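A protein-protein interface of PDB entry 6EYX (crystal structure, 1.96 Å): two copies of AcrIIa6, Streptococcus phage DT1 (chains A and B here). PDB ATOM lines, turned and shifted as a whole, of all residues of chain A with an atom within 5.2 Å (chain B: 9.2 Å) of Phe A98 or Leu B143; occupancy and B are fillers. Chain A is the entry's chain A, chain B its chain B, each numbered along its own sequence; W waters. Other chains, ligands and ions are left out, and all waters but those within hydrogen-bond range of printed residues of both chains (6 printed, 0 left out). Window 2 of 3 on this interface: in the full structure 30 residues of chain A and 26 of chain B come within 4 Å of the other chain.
The side-chain amino group of Lys A74 lies within salt-bridge range of the side-chain carboxylate of Asp B65 (2.8 Å). The backbone carbonyl oxygen of Tyr B148 is in hydrogen-bond range of the side-chain amino group of Lys A74 (2.8 Å). The side-chain amino group (NZ) of Lys A105 lies within hydrogen-bond range of the backbone carbonyl oxygen (O) of Ser B142.
OD1 of Asp B65 lies within hydrogen-bond range of N of Phe B67 (2.8 Å). OD2 of Asp B65 sits close to OE1 of Gln B151, at 2.8 Å. The backbone carbonyl oxygen of Ser B141 sits at hydrogen-bond distance from the backbone NH of Met B149. OG of Ser B142 sits at hydrogen-bond distance from N of Gly B144.
Among the printed residues, pairs that only touch across the chains: Met A71 with Met B149 (3.7 Å), Lys A74 with Asp B66 (3.8 Å), Lys A74 with Leu B143 (3.7 Å), Lys A74 with Met B149 (3.7 Å), Phe A98 with Leu B143 (3.6 Å), Phe A98 with Met B149 (3.8 Å) and Gln A102 with Met B149 (3.99 Å).
Of chain B, only Leu B143 (3.6 Å) and Met B149 (3.8 Å) come within 4 Å of Phe A98. Of chain A, only Lys A74 (3.7 Å) and Phe A98 (3.6 Å) come within 4 Å of Leu B143. Of the printed residues of chain A, Ser B142 touches Lys A105 (3.5 Å). Printed residues of chain A within 4 Å of Asp B65: Lys A74 (2.8 Å). Of the printed residues of chain B, Met A71 touches Met B149. Of the printed residues of chain B, Gln A102 touches Met B149. Ser B147 touches none of the printed residues of chain A. The nearest residue of chain B that does not touch Phe A98 is Ser B147 (7.0 Å). The nearest residue of chain A that does not touch Leu B143 is Gln A102 (4.1 Å).
Hydrophobic or aromatic side chains of chain B that line the printed part of chain A: Leu B143 and Met B149. Printed residues of chain A that touch a printed residue of chain B: Met A71, Lys A74, Phe A98, Gln A102 and Lys A105. Hydrophobic or aromatic side chains of chain A within 4 Å of the printed part of chain B: Met A71 and Phe A98. Among the printed residues, Asp or Glu carboxylates within 4 Å of a Lys or Arg side-chain nitrogen of the other chain: Lys A74 with Asp B65 (2.8 Å).
No position is printed for both chains. Of the 10 pairs that touch across the chains among the printed residues, none has its exchanged pair printed and touching as well.
Water W2 lies within hydrogen-bond range of OD1 of Asn A78, O of Lys A74 and OG of Ser B147. Water W5 lies within hydrogen-bond range of O of Ser B142 (2.7 Å), O of Ser B140 (2.7 Å) and NZ of Lys A105 (3.2 Å). Water W4 lies within hydrogen-bond range of OG of Ser B147 (2.7 Å), NZ of Lys A74 (2.8 Å), N of Tyr B148 (3.2 Å) and OE1 of Gln B151 (3.5 Å). Water W1 lies within hydrogen-bond range of the backbone carbonyl oxygen of Ser B141 (2.8 Å), the side-chain amide oxygen of Gln A102 (2.8 Å) and the side-chain amino group of Lys A105 (3.4 Å). Water W6 bridges N of Asp B66 (2.9 Å) and NZ of Lys A74 (3.0 Å). Water W3 bridges O of Ser B142 (3.3 Å) and NZ of Lys A105 (3.4 Å).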
ATOM      1  N   MET A  71      -4.014   0.830  14.713  1.00  0.00           N
ATOM      2  CA  MET A  71      -2.649   1.320  14.982  1.00  0.00           C
ATOM      3  C   MET A  71      -1.597   0.407  14.348  1.00  0.00           C
ATOM      4  O   MET A  71      -0.618   0.909  13.808  1.00  0.00           O
ATOM      5  CB  MET A  71      -2.376   1.476  16.485  1.00  0.00           C
ATOM      6  CG  MET A  71      -3.100   2.643  17.117  1.00  0.00           C
ATOM      7  SD  MET A  71      -2.376   3.154  18.709  1.00  0.00           S
ATOM      8  CE  MET A  71      -2.772   1.734  19.726  1.00  0.00           C
ATOM      9  N   LYS A  74      -1.548   1.315  10.598  1.00  0.00           N
ATOM     10  CA  LYS A  74      -0.926   2.639  10.401  1.00  0.00           C
ATOM     11  C   LYS A  74       0.604   2.549  10.665  1.00  0.00           C
ATOM     12  O   LYS A  74       1.385   3.142   9.914  1.00  0.00           O
ATOM     13  CB  LYS A  74      -1.571   3.692  11.334  1.00  0.00           C
ATOM     14  CG  LYS A  74      -3.082   3.918  11.134  1.00  0.00           C
ATOM     15  CD  LYS A  74      -3.431   4.760   9.921  1.00  0.00           C
ATOM     16  CE  LYS A  74      -4.937   4.852   9.762  1.00  0.00           C
ATOM     17  NZ  LYS A  74      -5.305   5.584   8.527  1.00  0.00           N
ATOM     18  N   ALA A  75       1.020   1.780  11.715  1.00  0.00           N
ATOM     19  CA  ALA A  75       2.433   1.572  12.066  1.00  0.00           C
ATOM     20  C   ALA A  75       3.166   0.868  10.908  1.00  0.00           C
ATOM     21  O   ALA A  75       4.257   1.305  10.544  1.00  0.00           O
ATOM     22  CB  ALA A  75       2.564   0.761  13.352  1.00  0.00           C
ATOM     23  N   ASN A  78       4.055   3.343   8.132  1.00  0.00           N
ATOM     24  CA  ASN A  78       5.221   4.117   8.568  1.00  0.00           C
ATOM     25  C   ASN A  78       6.504   3.298   8.466  1.00  0.00           C
ATOM     26  O   ASN A  78       7.471   3.767   7.883  1.00  0.00           O
ATOM     27  CB  ASN A  78       5.050   4.593  10.019  1.00  0.00           C
ATOM     28  CG  ASN A  78       4.148   5.787  10.214  1.00  0.00           C
ATOM     29  OD1 ASN A  78       3.534   6.312   9.279  1.00  0.00           O
ATOM     30  ND2 ASN A  78       4.049   6.242  11.451  1.00  0.00           N
ATOM     31  N   TYR A  94       8.705  -1.308  16.862  1.00  0.00           N
ATOM     32  CA  TYR A  94       8.242  -0.041  16.287  1.00  0.00           C
ATOM     33  C   TYR A  94       6.771   0.210  16.652  1.00  0.00           C
ATOM     34  O   TYR A  94       6.427   1.333  17.004  1.00  0.00           O
ATOM     35  CB  TYR A  94       8.444   0.073  14.763  1.00  0.00           C
ATOM     36  CG  TYR A  94       7.854   1.375  14.263  1.00  0.00           C
ATOM     37  CD1 TYR A  94       8.383   2.599  14.673  1.00  0.00           C
ATOM     38  CD2 TYR A  94       6.695   1.392  13.493  1.00  0.00           C
ATOM     39  CE1 TYR A  94       7.774   3.798  14.326  1.00  0.00           C
ATOM     40  CE2 TYR A  94       6.089   2.592  13.127  1.00  0.00           C
ATOM     41  CZ  TYR A  94       6.645   3.794  13.533  1.00  0.00           C
ATOM     42  OH  TYR A  94       6.078   4.987  13.187  1.00  0.00           O
ATOM     43  N   TYR A  95       5.920  -0.845  16.584  1.00  0.00           N
ATOM     44  CA  TYR A  95       4.500  -0.742  16.943  1.00  0.00           C
ATOM     45  C   TYR A  95       4.325  -0.230  18.395  1.00  0.00           C
ATOM     46  O   TYR A  95       3.493   0.653  18.608  1.00  0.00           O
ATOM     47  CB  TYR A  95       3.726  -2.071  16.694  1.00  0.00           C
ATOM     48  CG  TYR A  95       2.424  -2.131  17.469  1.00  0.00           C
ATOM     49  CD1 TYR A  95       1.318  -1.375  17.066  1.00  0.00           C
ATOM     50  CD2 TYR A  95       2.330  -2.841  18.662  1.00  0.00           C
ATOM     51  CE1 TYR A  95       0.153  -1.331  17.836  1.00  0.00           C
ATOM     52  CE2 TYR A  95       1.164  -2.820  19.429  1.00  0.00           C
ATOM     53  CZ  TYR A  95       0.070  -2.082  18.998  1.00  0.00           C
ATOM     54  OH  TYR A  95      -1.081  -2.047  19.751  1.00  0.00           O
ATOM     55  N   ASP A  96       5.118  -0.767  19.374  1.00  0.00           N
ATOM     56  CA  ASP A  96       5.088  -0.329  20.788  1.00  0.00           C
ATOM     57  C   ASP A  96       5.419   1.148  20.914  1.00  0.00           C
ATOM     58  O   ASP A  96       4.818   1.858  21.726  1.00  0.00           O
ATOM     59  CB  ASP A  96       6.037  -1.166  21.668  1.00  0.00           C
ATOM     60  CG  ASP A  96       5.469  -2.521  22.047  1.00  0.00           C
ATOM     61  OD1 ASP A  96       4.385  -2.858  21.564  1.00  0.00           O
ATOM     62  OD2 ASP A  96       6.088  -3.211  22.862  1.00  0.00           O
ATOM     63  N   MET A  97       6.376   1.599  20.101  1.00  0.00           N
ATOM     64  CA  MET A  97       6.795   2.991  20.048  1.00  0.00           C
ATOM     65  C   MET A  97       5.652   3.859  19.459  1.00  0.00           C
ATOM     66  O   MET A  97       5.380   4.937  19.991  1.00  0.00           O
ATOM     67  CB  MET A  97       8.080   3.096  19.218  1.00  0.00           C
ATOM     68  CG  MET A  97       8.649   4.477  19.146  1.00  0.00           C
ATOM     69  SD  MET A  97      10.297   4.375  18.426  1.00  0.00           S
ATOM     70  CE  MET A  97      10.582   6.092  18.042  1.00  0.00           C
ATOM     71  N   PHE A  98       5.006   3.391  18.357  1.00  0.00           N
ATOM     72  CA  PHE A  98       3.876   4.087  17.706  1.00  0.00           C
ATOM     73  C   PHE A  98       2.737   4.235  18.726  1.00  0.00           C
ATOM     74  O   PHE A  98       2.170   5.319  18.875  1.00  0.00           O
ATOM     75  CB  PHE A  98       3.413   3.303  16.452  1.00  0.00           C
ATOM     76  CG  PHE A  98       2.258   3.910  15.682  1.00  0.00           C
ATOM     77  CD1 PHE A  98       0.945   3.734  16.113  1.00  0.00           C
ATOM     78  CD2 PHE A  98       2.476   4.610  14.501  1.00  0.00           C
ATOM     79  CE1 PHE A  98      -0.121   4.314  15.419  1.00  0.00           C
ATOM     80  CE2 PHE A  98       1.401   5.175  13.792  1.00  0.00           C
ATOM     81  CZ  PHE A  98       0.113   5.045  14.268  1.00  0.00           C
ATOM     82  N   LYS A  99       2.418   3.136  19.437  1.00  0.00           N
ATOM     83  CA  LYS A  99       1.361   3.094  20.441  1.00  0.00           C
ATOM     84  C   LYS A  99       1.660   4.057  21.602  1.00  0.00           C
ATOM     85  O   LYS A  99       0.768   4.794  22.031  1.00  0.00           O
ATOM     86  CB  LYS A  99       1.167   1.637  20.946  1.00  0.00           C
ATOM     87  CG  LYS A  99       0.183   1.503  22.122  1.00  0.00           C
ATOM     88  CD  LYS A  99      -0.015   0.053  22.582  1.00  0.00           C
ATOM     89  CE  LYS A  99       1.212  -0.530  23.240  1.00  0.00           C
ATOM     90  NZ  LYS A  99       0.939  -1.835  23.910  1.00  0.00           N
ATOM     91  N   LYS A 100       2.923   4.059  22.098  1.00  0.00           N
ATOM     92  CA  LYS A 100       3.349   4.948  23.182  1.00  0.00           C
ATOM     93  C   LYS A 100       3.194   6.413  22.744  1.00  0.00           C
ATOM     94  O   LYS A 100       2.749   7.248  23.544  1.00  0.00           O
ATOM     95  CB  LYS A 100       4.831   4.668  23.568  1.00  0.00           C
ATOM     96  CG  LYS A 100       5.406   5.561  24.698  1.00  0.00           C
ATOM     97  CD  LYS A 100       4.705   5.420  26.090  1.00  0.00           C
ATOM     98  CE  LYS A 100       4.699   3.998  26.642  1.00  0.00           C
ATOM     99  NZ  LYS A 100       6.071   3.551  26.994  1.00  0.00           N
ATOM    100  N   GLN A 101       3.545   6.715  21.480  1.00  0.00           N
ATOM    101  CA  GLN A 101       3.423   8.088  20.957  1.00  0.00           C
ATOM    102  C   GLN A 101       1.959   8.517  20.871  1.00  0.00           C
ATOM    103  O   GLN A 101       1.666   9.683  21.122  1.00  0.00           O
ATOM    104  CB  GLN A 101       4.174   8.265  19.628  1.00  0.00           C
ATOM    105  CG  GLN A 101       5.715   8.264  19.775  1.00  0.00           C
ATOM    106  CD  GLN A 101       6.274   9.247  20.795  1.00  0.00           C
ATOM    107  OE1 GLN A 101       6.991   8.867  21.719  1.00  0.00           O
ATOM    108  NE2 GLN A 101       5.958  10.535  20.671  1.00  0.00           N
ATOM    109  N   GLN A 102       1.039   7.560  20.599  1.00  0.00           N
ATOM    110  CA  GLN A 102      -0.407   7.818  20.553  1.00  0.00           C
ATOM    111  C   GLN A 102      -0.888   8.201  21.967  1.00  0.00           C
ATOM    112  O   GLN A 102      -1.611   9.178  22.099  1.00  0.00           O
ATOM    113  CB  GLN A 102      -1.175   6.574  20.069  1.00  0.00           C
ATOM    114  CG  GLN A 102      -1.707   6.570  18.640  1.00  0.00           C
ATOM    115  CD  GLN A 102      -2.232   7.873  18.101  1.00  0.00           C
ATOM    116  OE1 GLN A 102      -1.621   8.426  17.205  1.00  0.00           O
ATOM    117  NE2 GLN A 102      -3.393   8.345  18.538  1.00  0.00           N
ATOM    118  N   LYS A 105       0.230  11.698  22.859  1.00  0.00           N
ATOM    119  CA  LYS A 105      -0.642  12.624  22.127  1.00  0.00           C
ATOM    120  C   LYS A 105      -1.952  12.855  22.899  1.00  0.00           C
ATOM    121  O   LYS A 105      -2.373  13.996  23.051  1.00  0.00           O
ATOM    122  CB  LYS A 105      -0.944  12.061  20.740  1.00  0.00           C
ATOM    123  CG  LYS A 105      -1.056  13.100  19.649  1.00  0.00           C
ATOM    124  CD  LYS A 105       0.017  12.843  18.613  1.00  0.00           C
ATOM    125  CE  LYS A 105      -0.506  12.634  17.227  1.00  0.00           C
ATOM    126  NZ  LYS A 105       0.560  12.124  16.320  1.00  0.00           N
ATOM    127  N   ASP B  65     -10.045   2.115   5.202  1.00  0.00           N
ATOM    128  CA  ASP B  65      -8.947   2.750   5.897  1.00  0.00           C
ATOM    129  C   ASP B  65      -8.720   1.901   7.156  1.00  0.00           C
ATOM    130  O   ASP B  65      -9.670   1.268   7.631  1.00  0.00           O
ATOM    131  CB  ASP B  65      -9.349   4.164   6.318  1.00  0.00           C
ATOM    132  CG  ASP B  65      -8.219   4.945   6.945  1.00  0.00           C
ATOM    133  OD1 ASP B  65      -8.006   4.806   8.185  1.00  0.00           O
ATOM    134  OD2 ASP B  65      -7.581   5.743   6.224  1.00  0.00           O
ATOM    135  N   ASP B  66      -7.483   1.872   7.688  1.00  0.00           N
ATOM    136  CA  ASP B  66      -7.197   1.108   8.912  1.00  0.00           C
ATOM    137  C   ASP B  66      -8.104   1.538  10.072  1.00  0.00           C
ATOM    138  O   ASP B  66      -8.522   0.689  10.838  1.00  0.00           O
ATOM    139  CB  ASP B  66      -5.718   1.184   9.315  1.00  0.00           C
ATOM    140  CG  ASP B  66      -4.832   0.283   8.475  1.00  0.00           C
ATOM    141  OD1 ASP B  66      -5.026  -0.949   8.519  1.00  0.00           O
ATOM    142  OD2 ASP B  66      -3.972   0.808   7.758  1.00  0.00           O
ATOM    143  N   PHE B  67      -8.459   2.832  10.160  1.00  0.00           N
ATOM    144  CA  PHE B  67      -9.381   3.275  11.224  1.00  0.00           C
ATOM    145  C   PHE B  67     -10.796   2.678  11.005  1.00  0.00           C
ATOM    146  O   PHE B  67     -11.473   2.331  11.976  1.00  0.00           O
ATOM    147  CB  PHE B  67      -9.432   4.805  11.348  1.00  0.00           C
ATOM    148  CG  PHE B  67     -10.425   5.279  12.395  1.00  0.00           C
ATOM    149  CD1 PHE B  67     -10.153   5.126  13.752  1.00  0.00           C
ATOM    150  CD2 PHE B  67     -11.652   5.824  12.025  1.00  0.00           C
ATOM    151  CE1 PHE B  67     -11.095   5.517  14.719  1.00  0.00           C
ATOM    152  CE2 PHE B  67     -12.582   6.231  12.995  1.00  0.00           C
ATOM    153  CZ  PHE B  67     -12.285   6.097  14.333  1.00  0.00           C
ATOM    154  N   ALA B 137     -11.144  13.196   7.659  1.00  0.00           N
ATOM    155  CA  ALA B 137     -10.188  12.919   8.731  1.00  0.00           C
ATOM    156  C   ALA B 137     -10.167  14.002   9.799  1.00  0.00           C
ATOM    157  O   ALA B 137     -10.667  15.111   9.578  1.00  0.00           O
ATOM    158  CB  ALA B 137      -8.790  12.742   8.148  1.00  0.00           C
ATOM    159  N   LEU B 138      -9.600  13.670  10.965  1.00  0.00           N
ATOM    160  CA  LEU B 138      -9.373  14.636  12.028  1.00  0.00           C
ATOM    161  C   LEU B 138      -7.922  15.084  11.856  1.00  0.00           C
ATOM    162  O   LEU B 138      -7.006  14.267  11.932  1.00  0.00           O
ATOM    163  CB  LEU B 138      -9.633  14.058  13.438  1.00  0.00           C
ATOM    164  CG  LEU B 138     -11.097  13.733  13.807  1.00  0.00           C
ATOM    165  CD1 LEU B 138     -11.217  13.380  15.263  1.00  0.00           C
ATOM    166  CD2 LEU B 138     -12.028  14.903  13.537  1.00  0.00           C
ATOM    167  N   GLU B 139      -7.725  16.370  11.524  1.00  0.00           N
ATOM    168  CA  GLU B 139      -6.413  16.957  11.271  1.00  0.00           C
ATOM    169  C   GLU B 139      -5.393  16.700  12.402  1.00  0.00           C
ATOM    170  O   GLU B 139      -4.251  16.330  12.124  1.00  0.00           O
ATOM    171  CB  GLU B 139      -6.555  18.462  10.949  1.00  0.00           C
ATOM    172  CG  GLU B 139      -5.228  19.197  10.880  1.00  0.00           C
ATOM    173  CD  GLU B 139      -5.282  20.540  10.194  1.00  0.00           C
ATOM    174  OE1 GLU B 139      -5.124  20.549   8.953  1.00  0.00           O
ATOM    175  OE2 GLU B 139      -5.489  21.570  10.874  1.00  0.00           O
ATOM    176  N   SER B 140      -5.825  16.854  13.669  1.00  0.00           N
ATOM    177  CA  SER B 140      -5.010  16.643  14.857  1.00  0.00           C
ATOM    178  C   SER B 140      -4.484  15.210  14.969  1.00  0.00           C
ATOM    179  O   SER B 140      -3.508  15.001  15.678  1.00  0.00           O
ATOM    180  CB  SER B 140      -5.763  17.053  16.122  1.00  0.00           C
ATOM    181  OG  SER B 140      -6.811  16.154  16.447  1.00  0.00           O
ATOM    182  N   SER B 141      -5.094  14.244  14.239  1.00  0.00           N
ATOM    183  CA  SER B 141      -4.673  12.833  14.241  1.00  0.00           C
ATOM    184  C   SER B 141      -3.586  12.539  13.180  1.00  0.00           C
ATOM    185  O   SER B 141      -3.229  11.374  12.979  1.00  0.00           O
ATOM    186  CB  SER B 141      -5.878  11.904  14.084  1.00  0.00           C
ATOM    187  OG  SER B 141      -6.336  11.797  12.745  1.00  0.00           O
ATOM    188  N   SER B 142      -3.052  13.594  12.521  1.00  0.00           N
ATOM    189  CA  SER B 142      -2.024  13.473  11.476  1.00  0.00           C
ATOM    190  C   SER B 142      -0.847  12.582  11.880  1.00  0.00           C
ATOM    191  O   SER B 142      -0.360  12.679  13.001  1.00  0.00           O
ATOM    192  CB  SER B 142      -1.512  14.850  11.058  1.00  0.00           C
ATOM    193  OG  SER B 142      -0.511  14.723  10.059  1.00  0.00           O
ATOM    194  N   LEU B 143      -0.419  11.696  10.976  1.00  0.00           N
ATOM    195  CA  LEU B 143       0.705  10.788  11.206  1.00  0.00           C
ATOM    196  C   LEU B 143       1.889  11.152  10.298  1.00  0.00           C
ATOM    197  O   LEU B 143       2.914  10.460  10.304  1.00  0.00           O
ATOM    198  CB  LEU B 143       0.276   9.322  10.984  1.00  0.00           C
ATOM    199  CG  LEU B 143      -0.751   8.753  11.977  1.00  0.00           C
ATOM    200  CD1 LEU B 143      -1.313   7.435  11.474  1.00  0.00           C
ATOM    201  CD2 LEU B 143      -0.144   8.571  13.371  1.00  0.00           C
ATOM    202  N   GLY B 144       1.727  12.243   9.544  1.00  0.00           N
ATOM    203  CA  GLY B 144       2.704  12.732   8.580  1.00  0.00           C
ATOM    204  C   GLY B 144       2.560  12.025   7.243  1.00  0.00           C
ATOM    205  O   GLY B 144       2.014  10.919   7.185  1.00  0.00           O
ATOM    206  N   SER B 145       3.045  12.666   6.158  1.00  0.00           N
ATOM    207  CA  SER B 145       3.031  12.155   4.773  1.00  0.00           C
ATOM    208  C   SER B 145       1.627  11.745   4.265  1.00  0.00           C
ATOM    209  O   SER B 145       1.465  10.680   3.657  1.00  0.00           O
ATOM    210  CB  SER B 145       4.040  11.016   4.597  1.00  0.00           C
ATOM    211  OG  SER B 145       5.320  11.338   5.118  1.00  0.00           O
ATOM    212  N   GLY B 146       0.633  12.599   4.530  1.00  0.00           N
ATOM    213  CA  GLY B 146      -0.760  12.404   4.132  1.00  0.00           C
ATOM    214  C   GLY B 146      -1.500  11.286   4.849  1.00  0.00           C
ATOM    215  O   GLY B 146      -2.556  10.848   4.384  1.00  0.00           O
ATOM    216  N   SER B 147      -0.953  10.808   5.978  1.00  0.00           N
ATOM    217  CA  SER B 147      -1.553   9.738   6.773  1.00  0.00           C
ATOM    218  C   SER B 147      -2.190  10.332   8.031  1.00  0.00           C
ATOM    219  O   SER B 147      -1.699  11.334   8.556  1.00  0.00           O
ATOM    220  CB  SER B 147      -0.507   8.679   7.121  1.00  0.00           C
ATOM    221  OG  SER B 147      -1.084   7.544   7.741  1.00  0.00           O
ATOM    222  N   TYR B 148      -3.328   9.763   8.464  1.00  0.00           N
ATOM    223  CA  TYR B 148      -4.078  10.234   9.630  1.00  0.00           C
ATOM    224  C   TYR B 148      -4.520   9.034  10.440  1.00  0.00           C
ATOM    225  O   TYR B 148      -4.868   8.022   9.851  1.00  0.00           O
ATOM    226  CB  TYR B 148      -5.305  11.068   9.194  1.00  0.00           C
ATOM    227  CG  TYR B 148      -4.933  12.369   8.504  1.00  0.00           C
ATOM    228  CD1 TYR B 148      -4.708  12.396   7.123  1.00  0.00           C
ATOM    229  CD2 TYR B 148      -4.761  13.541   9.212  1.00  0.00           C
ATOM    230  CE1 TYR B 148      -4.304  13.570   6.486  1.00  0.00           C
ATOM    231  CE2 TYR B 148      -4.364  14.722   8.587  1.00  0.00           C
ATOM    232  CZ  TYR B 148      -4.143  14.729   7.219  1.00  0.00           C
ATOM    233  OH  TYR B 148      -3.760  15.880   6.584  1.00  0.00           O
ATOM    234  N   MET B 149      -4.484   9.131  11.779  1.00  0.00           N
ATOM    235  CA  MET B 149      -4.911   8.008  12.633  1.00  0.00           C
ATOM    236  C   MET B 149      -6.436   7.822  12.551  1.00  0.00           C
ATOM    237  O   MET B 149      -6.908   6.679  12.521  1.00  0.00           O
ATOM    238  CB  MET B 149      -4.434   8.214  14.086  1.00  0.00           C
ATOM    239  CG  MET B 149      -4.652   7.005  14.999  1.00  0.00           C
ATOM    240  SD  MET B 149      -3.686   5.541  14.541  1.00  0.00           S
ATOM    241  CE  MET B 149      -5.013   4.364  14.269  1.00  0.00           C
ATOM    242  N   LEU B 150      -7.199   8.942  12.544  1.00  0.00           N
ATOM    243  CA  LEU B 150      -8.665   8.925  12.472  1.00  0.00           C
ATOM    244  C   LEU B 150      -9.076   9.399  11.082  1.00  0.00           C
ATOM    245  O   LEU B 150      -8.933  10.583  10.746  1.00  0.00           O
ATOM    246  CB  LEU B 150      -9.320   9.805  13.567  1.00  0.00           C
ATOM    247  CG  LEU B 150      -9.085   9.514  15.075  1.00  0.00           C
ATOM    248  CD1 LEU B 150     -10.328   9.816  15.874  1.00  0.00           C
ATOM    249  CD2 LEU B 150      -8.619   8.095  15.374  1.00  0.00           C
ATOM    250  N   GLN B 151      -9.525   8.454  10.264  1.00  0.00           N
ATOM    251  CA  GLN B 151      -9.896   8.690   8.885  1.00  0.00           C
ATOM    252  C   GLN B 151     -11.003   7.727   8.449  1.00  0.00           C
ATOM    253  O   GLN B 151     -10.977   6.552   8.812  1.00  0.00           O
ATOM    254  CB  GLN B 151      -8.648   8.551   7.998  1.00  0.00           C
ATOM    255  CG  GLN B 151      -8.841   9.015   6.566  1.00  0.00           C
ATOM    256  CD  GLN B 151      -7.507   9.275   5.922  1.00  0.00           C
ATOM    257  OE1 GLN B 151      -6.656   8.393   5.782  1.00  0.00           O
ATOM    258  NE2 GLN B 151      -7.276  10.509   5.560  1.00  0.00           N
HETATM  259  O   HOH W   1      -2.308  10.578  15.488  1.00  0.00           O
HETATM  260  O   HOH W   2       0.874   5.764   9.128  1.00  0.00           O
HETATM  261  O   HOH W   3       2.763  13.016  13.910  1.00  0.00           O
HETATM  262  O   HOH W   4      -3.601   7.033   6.808  1.00  0.00           O
HETATM  263  O   HOH W   5      -0.921  14.539  14.906  1.00  0.00           O
HETATM  264  O   HOH W   6      -5.153   3.206   6.682  1.00  0.00           O
